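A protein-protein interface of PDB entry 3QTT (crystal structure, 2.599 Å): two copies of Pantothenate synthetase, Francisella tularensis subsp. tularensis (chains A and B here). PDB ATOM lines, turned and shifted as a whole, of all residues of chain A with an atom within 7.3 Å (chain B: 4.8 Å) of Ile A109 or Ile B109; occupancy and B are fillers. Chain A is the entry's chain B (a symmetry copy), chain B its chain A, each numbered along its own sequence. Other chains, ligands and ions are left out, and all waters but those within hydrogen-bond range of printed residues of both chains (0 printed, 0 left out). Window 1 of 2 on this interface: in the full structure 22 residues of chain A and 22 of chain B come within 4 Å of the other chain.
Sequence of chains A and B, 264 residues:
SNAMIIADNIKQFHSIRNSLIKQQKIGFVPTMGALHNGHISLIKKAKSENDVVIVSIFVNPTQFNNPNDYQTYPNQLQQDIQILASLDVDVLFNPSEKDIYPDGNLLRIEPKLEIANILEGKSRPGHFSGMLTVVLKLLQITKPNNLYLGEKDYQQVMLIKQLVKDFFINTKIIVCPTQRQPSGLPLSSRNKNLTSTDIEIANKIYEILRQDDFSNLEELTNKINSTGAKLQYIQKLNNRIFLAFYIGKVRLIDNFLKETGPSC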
ATOM      1  N   ASN A 105     -15.930 -31.274  10.077  1.00  0.00           N
ATOM      2  CA  ASN A 105     -16.509 -29.948   9.880  1.00  0.00           C
ATOM      3  C   ASN A 105     -17.103 -29.440  11.203  1.00  0.00           C
ATOM      4  O   ASN A 105     -18.301 -29.527  11.431  1.00  0.00           O
ATOM      5  CB  ASN A 105     -17.653 -30.121   8.870  1.00  0.00           C
ATOM      6  CG  ASN A 105     -18.203 -28.806   8.351  1.00  0.00           C
ATOM      7  OD1 ASN A 105     -17.581 -27.740   8.458  1.00  0.00           O
ATOM      8  ND2 ASN A 105     -19.380 -28.880   7.772  1.00  0.00           N
ATOM      9  N   LEU A 106     -16.261 -28.736  11.959  1.00  0.00           N
ATOM     10  CA  LEU A 106     -16.576 -28.224  13.292  1.00  0.00           C
ATOM     11  C   LEU A 106     -17.179 -26.844  13.350  1.00  0.00           C
ATOM     12  O   LEU A 106     -18.066 -26.560  14.159  1.00  0.00           O
ATOM     13  CB  LEU A 106     -15.406 -28.396  14.282  1.00  0.00           C
ATOM     14  CG  LEU A 106     -15.210 -29.826  14.828  1.00  0.00           C
ATOM     15  CD1 LEU A 106     -16.357 -30.775  14.444  1.00  0.00           C
ATOM     16  CD2 LEU A 106     -13.881 -30.408  14.421  1.00  0.00           C
ATOM     17  N   LEU A 107     -16.620 -25.968  12.524  1.00  0.00           N
ATOM     18  CA  LEU A 107     -17.059 -24.592  12.501  1.00  0.00           C
ATOM     19  C   LEU A 107     -17.736 -24.263  11.163  1.00  0.00           C
ATOM     20  O   LEU A 107     -17.182 -24.507  10.089  1.00  0.00           O
ATOM     21  CB  LEU A 107     -15.875 -23.668  12.832  1.00  0.00           C
ATOM     22  CG  LEU A 107     -15.277 -24.089  14.187  1.00  0.00           C
ATOM     23  CD1 LEU A 107     -14.083 -23.270  14.623  1.00  0.00           C
ATOM     24  CD2 LEU A 107     -16.345 -24.106  15.275  1.00  0.00           C
ATOM     25  N   ARG A 108     -18.964 -23.764  11.226  1.00  0.00           N
ATOM     26  CA  ARG A 108     -19.698 -23.466   9.996  1.00  0.00           C
ATOM     27  C   ARG A 108     -20.039 -22.000   9.891  1.00  0.00           C
ATOM     28  O   ARG A 108     -20.342 -21.335  10.898  1.00  0.00           O
ATOM     29  CB  ARG A 108     -20.993 -24.263   9.914  1.00  0.00           C
ATOM     30  CG  ARG A 108     -20.805 -25.749   9.890  1.00  0.00           C
ATOM     31  CD  ARG A 108     -21.428 -26.351  11.109  1.00  0.00           C
ATOM     32  NE  ARG A 108     -20.961 -27.710  11.372  1.00  0.00           N
ATOM     33  CZ  ARG A 108     -21.427 -28.809  10.777  1.00  0.00           C
ATOM     34  NH1 ARG A 108     -22.362 -28.717   9.839  1.00  0.00           N
ATOM     35  NH2 ARG A 108     -20.952 -30.008  11.111  1.00  0.00           N
ATOM     36  N   ILE A 109     -19.966 -21.494   8.662  1.00  0.00           N
ATOM     37  CA  ILE A 109     -20.651 -20.265   8.337  1.00  0.00           C
ATOM     38  C   ILE A 109     -22.115 -20.642   8.182  1.00  0.00           C
ATOM     39  O   ILE A 109     -22.463 -21.550   7.399  1.00  0.00           O
ATOM     40  CB  ILE A 109     -20.181 -19.661   7.031  1.00  0.00           C
ATOM     41  CG1 ILE A 109     -18.703 -19.339   7.126  1.00  0.00           C
ATOM     42  CG2 ILE A 109     -20.994 -18.402   6.733  1.00  0.00           C
ATOM     43  CD1 ILE A 109     -18.378 -18.382   8.263  1.00  0.00           C
ATOM     44  N   GLU A 110     -22.953 -19.983   8.975  1.00  0.00           N
ATOM     45  CA  GLU A 110     -24.388 -20.072   8.842  1.00  0.00           C
ATOM     46  C   GLU A 110     -25.000 -18.702   8.485  1.00  0.00           C
ATOM     47  O   GLU A 110     -24.855 -17.737   9.250  1.00  0.00           O
ATOM     48  CB  GLU A 110     -24.982 -20.669  10.117  1.00  0.00           C
ATOM     49  CG  GLU A 110     -25.534 -22.086   9.897  1.00  0.00           C
ATOM     50  CD  GLU A 110     -26.695 -22.102   8.865  1.00  0.00           C
ATOM     51  OE1 GLU A 110     -27.820 -21.643   9.191  1.00  0.00           O
ATOM     52  OE2 GLU A 110     -26.481 -22.560   7.719  1.00  0.00           O
ATOM     53  N   PRO A 111     -25.583 -18.586   7.271  1.00  0.00           N
ATOM     54  CA  PRO A 111     -26.311 -17.385   6.815  1.00  0.00           C
ATOM     55  C   PRO A 111     -27.652 -17.157   7.477  1.00  0.00           C
ATOM     56  O   PRO A 111     -28.422 -18.092   7.396  1.00  0.00           O
ATOM     57  CB  PRO A 111     -26.547 -17.667   5.324  1.00  0.00           C
ATOM     58  CG  PRO A 111     -26.463 -19.141   5.158  1.00  0.00           C
ATOM     59  CD  PRO A 111     -25.609 -19.679   6.278  1.00  0.00           C
ATOM     60  N   LYS A 112     -27.957 -15.984   8.046  1.00  0.00           N
ATOM     61  CA  LYS A 112     -29.356 -15.612   8.267  1.00  0.00           C
ATOM     62  C   LYS A 112     -29.660 -14.366   7.484  1.00  0.00           C
ATOM     63  O   LYS A 112     -29.377 -13.272   7.923  1.00  0.00           O
ATOM     64  CB  LYS A 112     -29.643 -15.340   9.743  1.00  0.00           C
ATOM     65  CG  LYS A 112     -29.863 -16.594  10.578  1.00  0.00           C
ATOM     66  CD  LYS A 112     -28.580 -17.407  10.695  1.00  0.00           C
ATOM     67  CE  LYS A 112     -28.786 -18.696  11.461  1.00  0.00           C
ATOM     68  NZ  LYS A 112     -27.466 -19.204  11.923  1.00  0.00           N
ATOM     69  N   GLY A 126     -28.608 -26.783   3.932  1.00  0.00           N
ATOM     70  CA  GLY A 126     -27.251 -27.022   4.401  1.00  0.00           C
ATOM     71  C   GLY A 126     -26.235 -26.553   3.391  1.00  0.00           C
ATOM     72  O   GLY A 126     -25.096 -26.277   3.746  1.00  0.00           O
ATOM     73  N   PHE A 128     -25.752 -23.862   1.342  1.00  0.00           N
ATOM     74  CA  PHE A 128     -25.154 -22.530   1.411  1.00  0.00           C
ATOM     75  C   PHE A 128     -24.133 -22.373   2.555  1.00  0.00           C
ATOM     76  O   PHE A 128     -23.090 -21.736   2.386  1.00  0.00           O
ATOM     77  CB  PHE A 128     -26.240 -21.455   1.440  1.00  0.00           C
ATOM     78  CG  PHE A 128     -26.794 -21.095   0.067  1.00  0.00           C
ATOM     79  CD1 PHE A 128     -25.992 -21.157  -1.063  1.00  0.00           C
ATOM     80  CD2 PHE A 128     -28.109 -20.664  -0.082  1.00  0.00           C
ATOM     81  CE1 PHE A 128     -26.499 -20.803  -2.329  1.00  0.00           C
ATOM     82  CE2 PHE A 128     -28.619 -20.297  -1.332  1.00  0.00           C
ATOM     83  CZ  PHE A 128     -27.810 -20.365  -2.459  1.00  0.00           C
ATOM     84  N   SER A 129     -24.402 -22.998   3.692  1.00  0.00           N
ATOM     85  CA  SER A 129     -23.436 -23.022   4.784  1.00  0.00           C
ATOM     86  C   SER A 129     -22.178 -23.790   4.388  1.00  0.00           C
ATOM     87  O   SER A 129     -21.031 -23.402   4.698  1.00  0.00           O
ATOM     88  CB  SER A 129     -24.052 -23.654   6.035  1.00  0.00           C
ATOM     89  OG  SER A 129     -23.057 -24.259   6.833  1.00  0.00           O
ATOM     90  N   GLY A 130     -22.406 -24.905   3.714  1.00  0.00           N
ATOM     91  CA  GLY A 130     -21.310 -25.695   3.205  1.00  0.00           C
ATOM     92  C   GLY A 130     -20.394 -24.899   2.307  1.00  0.00           C
ATOM     93  O   GLY A 130     -19.186 -24.868   2.498  1.00  0.00           O
ATOM     94  N   MET A 131     -20.985 -24.234   1.323  1.00  0.00           N
ATOM     95  CA  MET A 131     -20.219 -23.484   0.353  1.00  0.00           C
ATOM     96  C   MET A 131     -19.497 -22.297   1.008  1.00  0.00           C
ATOM     97  O   MET A 131     -18.287 -22.088   0.811  1.00  0.00           O
ATOM     98  CB  MET A 131     -21.137 -23.063  -0.789  1.00  0.00           C
ATOM     99  CG  MET A 131     -20.534 -22.096  -1.780  1.00  0.00           C
ATOM    100  SD  MET A 131     -20.843 -20.204  -1.294  1.00  0.00           S
ATOM    101  CE  MET A 131     -22.791 -20.126  -1.348  1.00  0.00           C
ATOM    102  N   LEU A 132     -20.237 -21.535   1.801  1.00  0.00           N
ATOM    103  CA  LEU A 132     -19.647 -20.402   2.504  1.00  0.00           C
ATOM    104  C   LEU A 132     -18.407 -20.775   3.364  1.00  0.00           C
ATOM    105  O   LEU A 132     -17.371 -20.104   3.335  1.00  0.00           O
ATOM    106  CB  LEU A 132     -20.710 -19.707   3.347  1.00  0.00           C
ATOM    107  CG  LEU A 132     -21.676 -18.888   2.508  1.00  0.00           C
ATOM    108  CD1 LEU A 132     -22.609 -18.122   3.413  1.00  0.00           C
ATOM    109  CD2 LEU A 132     -20.883 -17.948   1.630  1.00  0.00           C
ATOM    110  N   THR A 133     -18.515 -21.856   4.117  1.00  0.00           N
ATOM    111  CA  THR A 133     -17.382 -22.378   4.853  1.00  0.00           C
ATOM    112  C   THR A 133     -16.166 -22.704   3.961  1.00  0.00           C
ATOM    113  O   THR A 133     -15.055 -22.282   4.265  1.00  0.00           O
ATOM    114  CB  THR A 133     -17.818 -23.615   5.647  1.00  0.00           C
ATOM    115  OG1 THR A 133     -18.978 -23.277   6.422  1.00  0.00           O
ATOM    116  CG2 THR A 133     -16.712 -24.087   6.554  1.00  0.00           C
ATOM    117  N   VAL A 134     -16.365 -23.442   2.867  1.00  0.00           N
ATOM    118  CA  VAL A 134     -15.236 -23.794   2.011  1.00  0.00           C
ATOM    119  C   VAL A 134     -14.644 -22.568   1.312  1.00  0.00           C
ATOM    120  O   VAL A 134     -13.426 -22.403   1.289  1.00  0.00           O
ATOM    121  CB  VAL A 134     -15.558 -24.980   1.017  1.00  0.00           C
ATOM    122  CG1 VAL A 134     -16.277 -24.511  -0.224  1.00  0.00           C
ATOM    123  CG2 VAL A 134     -14.293 -25.706   0.614  1.00  0.00           C
ATOM    124  N   LEU A 136     -14.667 -19.611   2.374  1.00  0.00           N
ATOM    125  CA  LEU A 136     -13.941 -18.832   3.362  1.00  0.00           C
ATOM    126  C   LEU A 136     -12.562 -19.429   3.548  1.00  0.00           C
ATOM    127  O   LEU A 136     -11.575 -18.715   3.543  1.00  0.00           O
ATOM    128  CB  LEU A 136     -14.678 -18.768   4.693  1.00  0.00           C
ATOM    129  CG  LEU A 136     -14.039 -17.942   5.822  1.00  0.00           C
ATOM    130  CD1 LEU A 136     -13.494 -16.605   5.344  1.00  0.00           C
ATOM    131  CD2 LEU A 136     -15.110 -17.701   6.853  1.00  0.00           C
ATOM    132  N   LYS A 137     -12.503 -20.744   3.704  1.00  0.00           N
ATOM    133  CA  LYS A 137     -11.224 -21.427   3.837  1.00  0.00           C
ATOM    134  C   LYS A 137     -10.394 -21.169   2.604  1.00  0.00           C
ATOM    135  O   LYS A 137      -9.249 -20.737   2.705  1.00  0.00           O
ATOM    136  CB  LYS A 137     -11.408 -22.921   4.064  1.00  0.00           C
ATOM    137  CG  LYS A 137     -11.625 -23.283   5.511  1.00  0.00           C
ATOM    138  CD  LYS A 137     -12.537 -24.514   5.699  1.00  0.00           C
ATOM    139  CE  LYS A 137     -12.065 -25.377   6.855  1.00  0.00           C
ATOM    140  NZ  LYS A 137     -12.862 -25.182   8.064  1.00  0.00           N
ATOM    141  N   LEU A 163     -20.020 -12.334   2.447  1.00  0.00           N
ATOM    142  CA  LEU A 163     -18.942 -13.023   3.169  1.00  0.00           C
ATOM    143  C   LEU A 163     -17.651 -12.221   3.178  1.00  0.00           C
ATOM    144  O   LEU A 163     -17.039 -12.037   4.218  1.00  0.00           O
ATOM    145  CB  LEU A 163     -18.645 -14.361   2.511  1.00  0.00           C
ATOM    146  CG  LEU A 163     -17.494 -15.166   3.114  1.00  0.00           C
ATOM    147  CD1 LEU A 163     -17.936 -15.827   4.423  1.00  0.00           C
ATOM    148  CD2 LEU A 163     -16.996 -16.231   2.150  1.00  0.00           C
ATOM    149  N   PHE A 167     -16.195 -10.444   6.636  1.00  0.00           N
ATOM    150  CA  PHE A 167     -14.916 -10.959   7.110  1.00  0.00           C
ATOM    151  C   PHE A 167     -13.657 -10.212   6.741  1.00  0.00           C
ATOM    152  O   PHE A 167     -12.556 -10.756   6.857  1.00  0.00           O
ATOM    153  CB  PHE A 167     -14.863 -12.470   6.999  1.00  0.00           C
ATOM    154  CG  PHE A 167     -15.946 -13.108   7.800  1.00  0.00           C
ATOM    155  CD1 PHE A 167     -15.935 -13.003   9.185  1.00  0.00           C
ATOM    156  CD2 PHE A 167     -17.022 -13.695   7.191  1.00  0.00           C
ATOM    157  CE1 PHE A 167     -16.949 -13.546   9.936  1.00  0.00           C
ATOM    158  CE2 PHE A 167     -18.037 -14.233   7.922  1.00  0.00           C
ATOM    159  CZ  PHE A 167     -18.000 -14.160   9.305  1.00  0.00           C
ATOM    160  N   LEU B 107     -24.054 -13.464   8.920  1.00  0.00           N
ATOM    161  CA  LEU B 107     -23.159 -14.573   8.680  1.00  0.00           C
ATOM    162  C   LEU B 107     -22.480 -14.869  10.007  1.00  0.00           C
ATOM    163  O   LEU B 107     -21.863 -13.993  10.608  1.00  0.00           O
ATOM    164  CB  LEU B 107     -22.143 -14.234   7.587  1.00  0.00           C
ATOM    165  CG  LEU B 107     -22.620 -14.030   6.132  1.00  0.00           C
ATOM    166  CD1 LEU B 107     -21.464 -13.651   5.200  1.00  0.00           C
ATOM    167  CD2 LEU B 107     -23.440 -15.216   5.544  1.00  0.00           C
ATOM    168  N   ARG B 108     -22.631 -16.097  10.486  1.00  0.00           N
ATOM    169  CA  ARG B 108     -22.229 -16.416  11.840  1.00  0.00           C
ATOM    170  C   ARG B 108     -21.477 -17.710  11.825  1.00  0.00           C
ATOM    171  O   ARG B 108     -21.748 -18.575  10.988  1.00  0.00           O
ATOM    172  CB  ARG B 108     -23.447 -16.598  12.727  1.00  0.00           C
ATOM    173  CG  ARG B 108     -24.552 -15.637  12.433  1.00  0.00           C
ATOM    174  CD  ARG B 108     -25.790 -16.082  13.132  1.00  0.00           C
ATOM    175  NE  ARG B 108     -26.876 -15.140  12.914  1.00  0.00           N
ATOM    176  CZ  ARG B 108     -27.858 -14.913  13.784  1.00  0.00           C
ATOM    177  NH1 ARG B 108     -27.878 -15.553  14.956  1.00  0.00           N
ATOM    178  NH2 ARG B 108     -28.815 -14.033  13.484  1.00  0.00           N
ATOM    179  N   ILE B 109     -20.527 -17.821  12.752  1.00  0.00           N
ATOM    180  CA  ILE B 109     -19.855 -19.065  13.034  1.00  0.00           C
ATOM    181  C   ILE B 109     -20.746 -19.867  13.947  1.00  0.00           C
ATOM    182  O   ILE B 109     -21.109 -19.415  15.020  1.00  0.00           O
ATOM    183  CB  ILE B 109     -18.547 -18.788  13.744  1.00  0.00           C
ATOM    184  CG1 ILE B 109     -17.664 -17.929  12.849  1.00  0.00           C
ATOM    185  CG2 ILE B 109     -17.846 -20.096  14.162  1.00  0.00           C
ATOM    186  CD1 ILE B 109     -16.908 -18.722  11.815  1.00  0.00           C
ATOM    187  N   GLU B 110     -21.116 -21.062  13.517  1.00  0.00           N
ATOM    188  CA  GLU B 110     -21.894 -21.935  14.373  1.00  0.00           C
ATOM    189  C   GLU B 110     -21.057 -23.168  14.683  1.00  0.00           C
ATOM    190  O   GLU B 110     -20.750 -23.942  13.776  1.00  0.00           O
ATOM    191  CB  GLU B 110     -23.213 -22.305  13.697  1.00  0.00           C
ATOM    192  CG  GLU B 110     -24.037 -21.093  13.247  1.00  0.00           C
ATOM    193  CD  GLU B 110     -24.850 -20.443  14.358  1.00  0.00           C
ATOM    194  OE1 GLU B 110     -24.556 -20.679  15.550  1.00  0.00           O
ATOM    195  OE2 GLU B 110     -25.794 -19.689  14.038  1.00  0.00           O
ATOM    196  N   PRO B 111     -20.630 -23.319  15.954  1.00  0.00           N
ATOM    197  CA  PRO B 111     -19.855 -24.487  16.386  1.00  0.00           C
ATOM    198  C   PRO B 111     -20.698 -25.740  16.493  1.00  0.00           C
ATOM    199  O   PRO B 111     -21.722 -25.684  17.166  1.00  0.00           O
ATOM    200  CB  PRO B 111     -19.379 -24.095  17.795  1.00  0.00           C
ATOM    201  CG  PRO B 111     -20.100 -22.875  18.172  1.00  0.00           C
ATOM    202  CD  PRO B 111     -21.091 -22.527  17.105  1.00  0.00           C
ATOM    203  N   SER B 129     -21.462 -18.914  19.371  1.00  0.00           N
ATOM    204  CA  SER B 129     -21.614 -18.443  18.007  1.00  0.00           C
ATOM    205  C   SER B 129     -21.152 -16.991  17.907  1.00  0.00           C
ATOM    206  O   SER B 129     -20.371 -16.624  17.005  1.00  0.00           O
ATOM    207  CB  SER B 129     -23.079 -18.550  17.594  1.00  0.00           C
ATOM    208  OG  SER B 129     -23.253 -18.308  16.226  1.00  0.00           O
ATOM    209  N   LEU B 132     -17.490 -16.336  18.644  1.00  0.00           N
ATOM    210  CA  LEU B 132     -16.689 -16.844  17.540  1.00  0.00           C
ATOM    211  C   LEU B 132     -16.813 -15.943  16.314  1.00  0.00           C
ATOM    212  O   LEU B 132     -15.844 -15.716  15.597  1.00  0.00           O
ATOM    213  CB  LEU B 132     -17.054 -18.276  17.196  1.00  0.00           C
ATOM    214  CG  LEU B 132     -16.504 -19.274  18.218  1.00  0.00           C
ATOM    215  CD1 LEU B 132     -16.936 -20.685  17.870  1.00  0.00           C
ATOM    216  CD2 LEU B 132     -14.998 -19.207  18.288  1.00  0.00           C
ATOM    217  N   THR B 133     -18.007 -15.407  16.091  1.00  0.00           N
ATOM    218  CA  THR B 133     -18.186 -14.509  14.981  1.00  0.00           C
ATOM    219  C   THR B 133     -17.367 -13.220  15.204  1.00  0.00           C
ATOM    220  O   THR B 133     -16.617 -12.787  14.318  1.00  0.00           O
ATOM    221  CB  THR B 133     -19.679 -14.236  14.687  1.00  0.00           C
ATOM    222  OG1 THR B 133     -20.279 -15.416  14.152  1.00  0.00           O
ATOM    223  CG2 THR B 133     -19.813 -13.194  13.626  1.00  0.00           C
ATOM    224  N   LEU B 136     -13.483 -13.848  15.096  1.00  0.00           N
ATOM    225  CA  LEU B 136     -13.033 -13.984  13.721  1.00  0.00           C
ATOM    226  C   LEU B 136     -12.883 -12.614  13.100  1.00  0.00           C
ATOM    227  O   LEU B 136     -11.832 -12.302  12.551  1.00  0.00           O
ATOM    228  CB  LEU B 136     -14.016 -14.796  12.897  1.00  0.00           C
ATOM    229  CG  LEU B 136     -13.596 -15.022  11.442  1.00  0.00           C
ATOM    230  CD1 LEU B 136     -12.187 -15.662  11.354  1.00  0.00           C
ATOM    231  CD2 LEU B 136     -14.622 -15.890  10.789  1.00  0.00           C
ATOM    232  N   LEU B 163     -10.806 -22.335  15.845  1.00  0.00           N
ATOM    233  CA  LEU B 163     -11.141 -21.296  14.892  1.00  0.00           C
ATOM    234  C   LEU B 163      -9.953 -20.846  14.063  1.00  0.00           C
ATOM    235  O   LEU B 163     -10.045 -20.759  12.836  1.00  0.00           O
ATOM    236  CB  LEU B 163     -11.718 -20.074  15.609  1.00  0.00           C
ATOM    237  CG  LEU B 163     -11.970 -18.883  14.688  1.00  0.00           C
ATOM    238  CD1 LEU B 163     -13.374 -18.959  14.045  1.00  0.00           C
ATOM    239  CD2 LEU B 163     -11.729 -17.533  15.388  1.00  0.00           C
ATOM    240  N   PHE B 167      -9.636 -21.821   9.940  1.00  0.00           N
ATOM    241  CA  PHE B 167      -9.657 -20.665   9.090  1.00  0.00           C
ATOM    242  C   PHE B 167      -8.328 -20.126   8.609  1.00  0.00           C
ATOM    243  O   PHE B 167      -8.240 -18.994   8.129  1.00  0.00           O
ATOM    244  CB  PHE B 167     -10.677 -19.658   9.575  1.00  0.00           C
ATOM    245  CG  PHE B 167     -12.068 -20.193   9.466  1.00  0.00           C
ATOM    246  CD1 PHE B 167     -12.695 -20.256   8.241  1.00  0.00           C
ATOM    247  CD2 PHE B 167     -12.693 -20.748  10.547  1.00  0.00           C
ATOM    248  CE1 PHE B 167     -13.948 -20.799   8.118  1.00  0.00           C
ATOM    249  CE2 PHE B 167     -13.955 -21.285  10.435  1.00  0.00           C
ATOM    250  CZ  PHE B 167     -14.587 -21.307   9.220  1.00  0.00           C
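The backbone carbonyl oxygen (O) of Arg B108 sits at hydrogen-bond distance from the backbone NH (N) of Glu A110, 2.7 Å away.
The backbone NH of Glu B110 lies within hydrogen-bond range of the backbone carbonyl oxygen of Arg A108.
The side-chain carboxylate of Glu B110 lies within salt-bridge range of the side-chain amino group of Lys A112 (2.7 Å).
The backbone carbonyl oxygen (O) of Arg A108 lies close to the backbone carbonyl oxygen (O) of Arg B108 (3.1 Å).
O of Ile B109 is in hydrogen-bond range of OG of Ser B129.
The side-chain hydroxyl (OG1) of Thr B133 lies within hydrogen-bond range of the backbone NH (N) of Ile B109 (2.8 Å).
The side-chain carboxylate (OE1) of Glu B110 sits at hydrogen-bond distance from the side-chain hydroxyl (OG) of Ser B129 (2.8 Å).
NH2 of Arg A108 lies within hydrogen-bond range of O of Asn A105 (2.7 Å).
O of Ile A109 sits at hydrogen-bond distance from OG of Ser A129 (2.8 Å).
N of Ile A109 sits at hydrogen-bond distance from OG1 of Thr A133 (3.0 Å).
Leu A107 touches Phe B167, but with the chains exchanged Phe A167 does not touch Leu B107 (4.1 Å).
Arg A108 touches its own counterpart, Arg B108.
Arg A108 touches Glu B110, and with the chains exchanged Glu A110 touches Arg B108.
Leu A132 touches Leu B107, but with the chains exchanged Leu A107 does not touch Leu B132 (4.3 Å).
Of the 21 pairs that touch across the chains among the printed residues, 15 have their exchanged pair printed and touching as well.
Among the printed residues, merely in contact across the chains: Arg A108 with Ile B109 (3.2 Å), Glu A110 with Glu B110 (3.3 Å), Leu A163 with Leu B107 (3.3 Å), Ile A109 with Arg B108 (3.3 Å), Phe A167 with Leu B136 (3.4 Å), Leu A106 with Pro B111 (3.5 Å), Leu A136 with Phe B167 (3.5 Å), Leu A107 with Leu B163 (3.6 Å), Lys A112 with Arg B108 (3.6 Å), Glu A110 with Leu B107 (3.6 Å), Leu A132 with Leu B107 (3.7 Å), Leu A107 with Pro B111 (3.7 Å), Leu A106 with Glu B110 (3.8 Å), Pro A111 with Leu B107 (3.8 Å), Ile A109 with Ile B109 (3.9 Å), Leu A107 with Phe B167 (3.9 Å) and Leu A107 with Glu B110 (3.96 Å).
Of the 11 printed residues of chain B, 8 touch a printed residue of chain A.
Hydrophobic or aromatic side chains of chain A that line the printed part of chain B: Leu A107, Ile A109, Pro A111, Leu A132, Leu A136, Leu A163 and Phe A167.
Among the printed residues, 21 pairs touch across the chains.
Among the printed residues, Asp or Glu carboxylates within 4 Å of a Lys or Arg side-chain nitrogen of the other chain: Lys A112 with Glu B110 (2.7 Å).
Of the printed residues of chain B, Ile A109 touches Arg B108 and Ile B109.
Printed residues of chain B within 4 Å of Lys A112: Arg B108 and Glu B110.
Of the printed residues of chain B, Leu A132 touches Leu B107.
Of chain A, only Arg A108 (3.2 Å) and Ile A109 (3.9 Å) come within 4 Å of Ile B109.
Leu B132 touches none of the printed residues of chain A.
Of the printed residues of chain A, Leu B136 touches Phe A167 (3.4 Å).
The nearest residue of chain B that does not touch Ile A109 is Leu B107 (4.2 Å).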
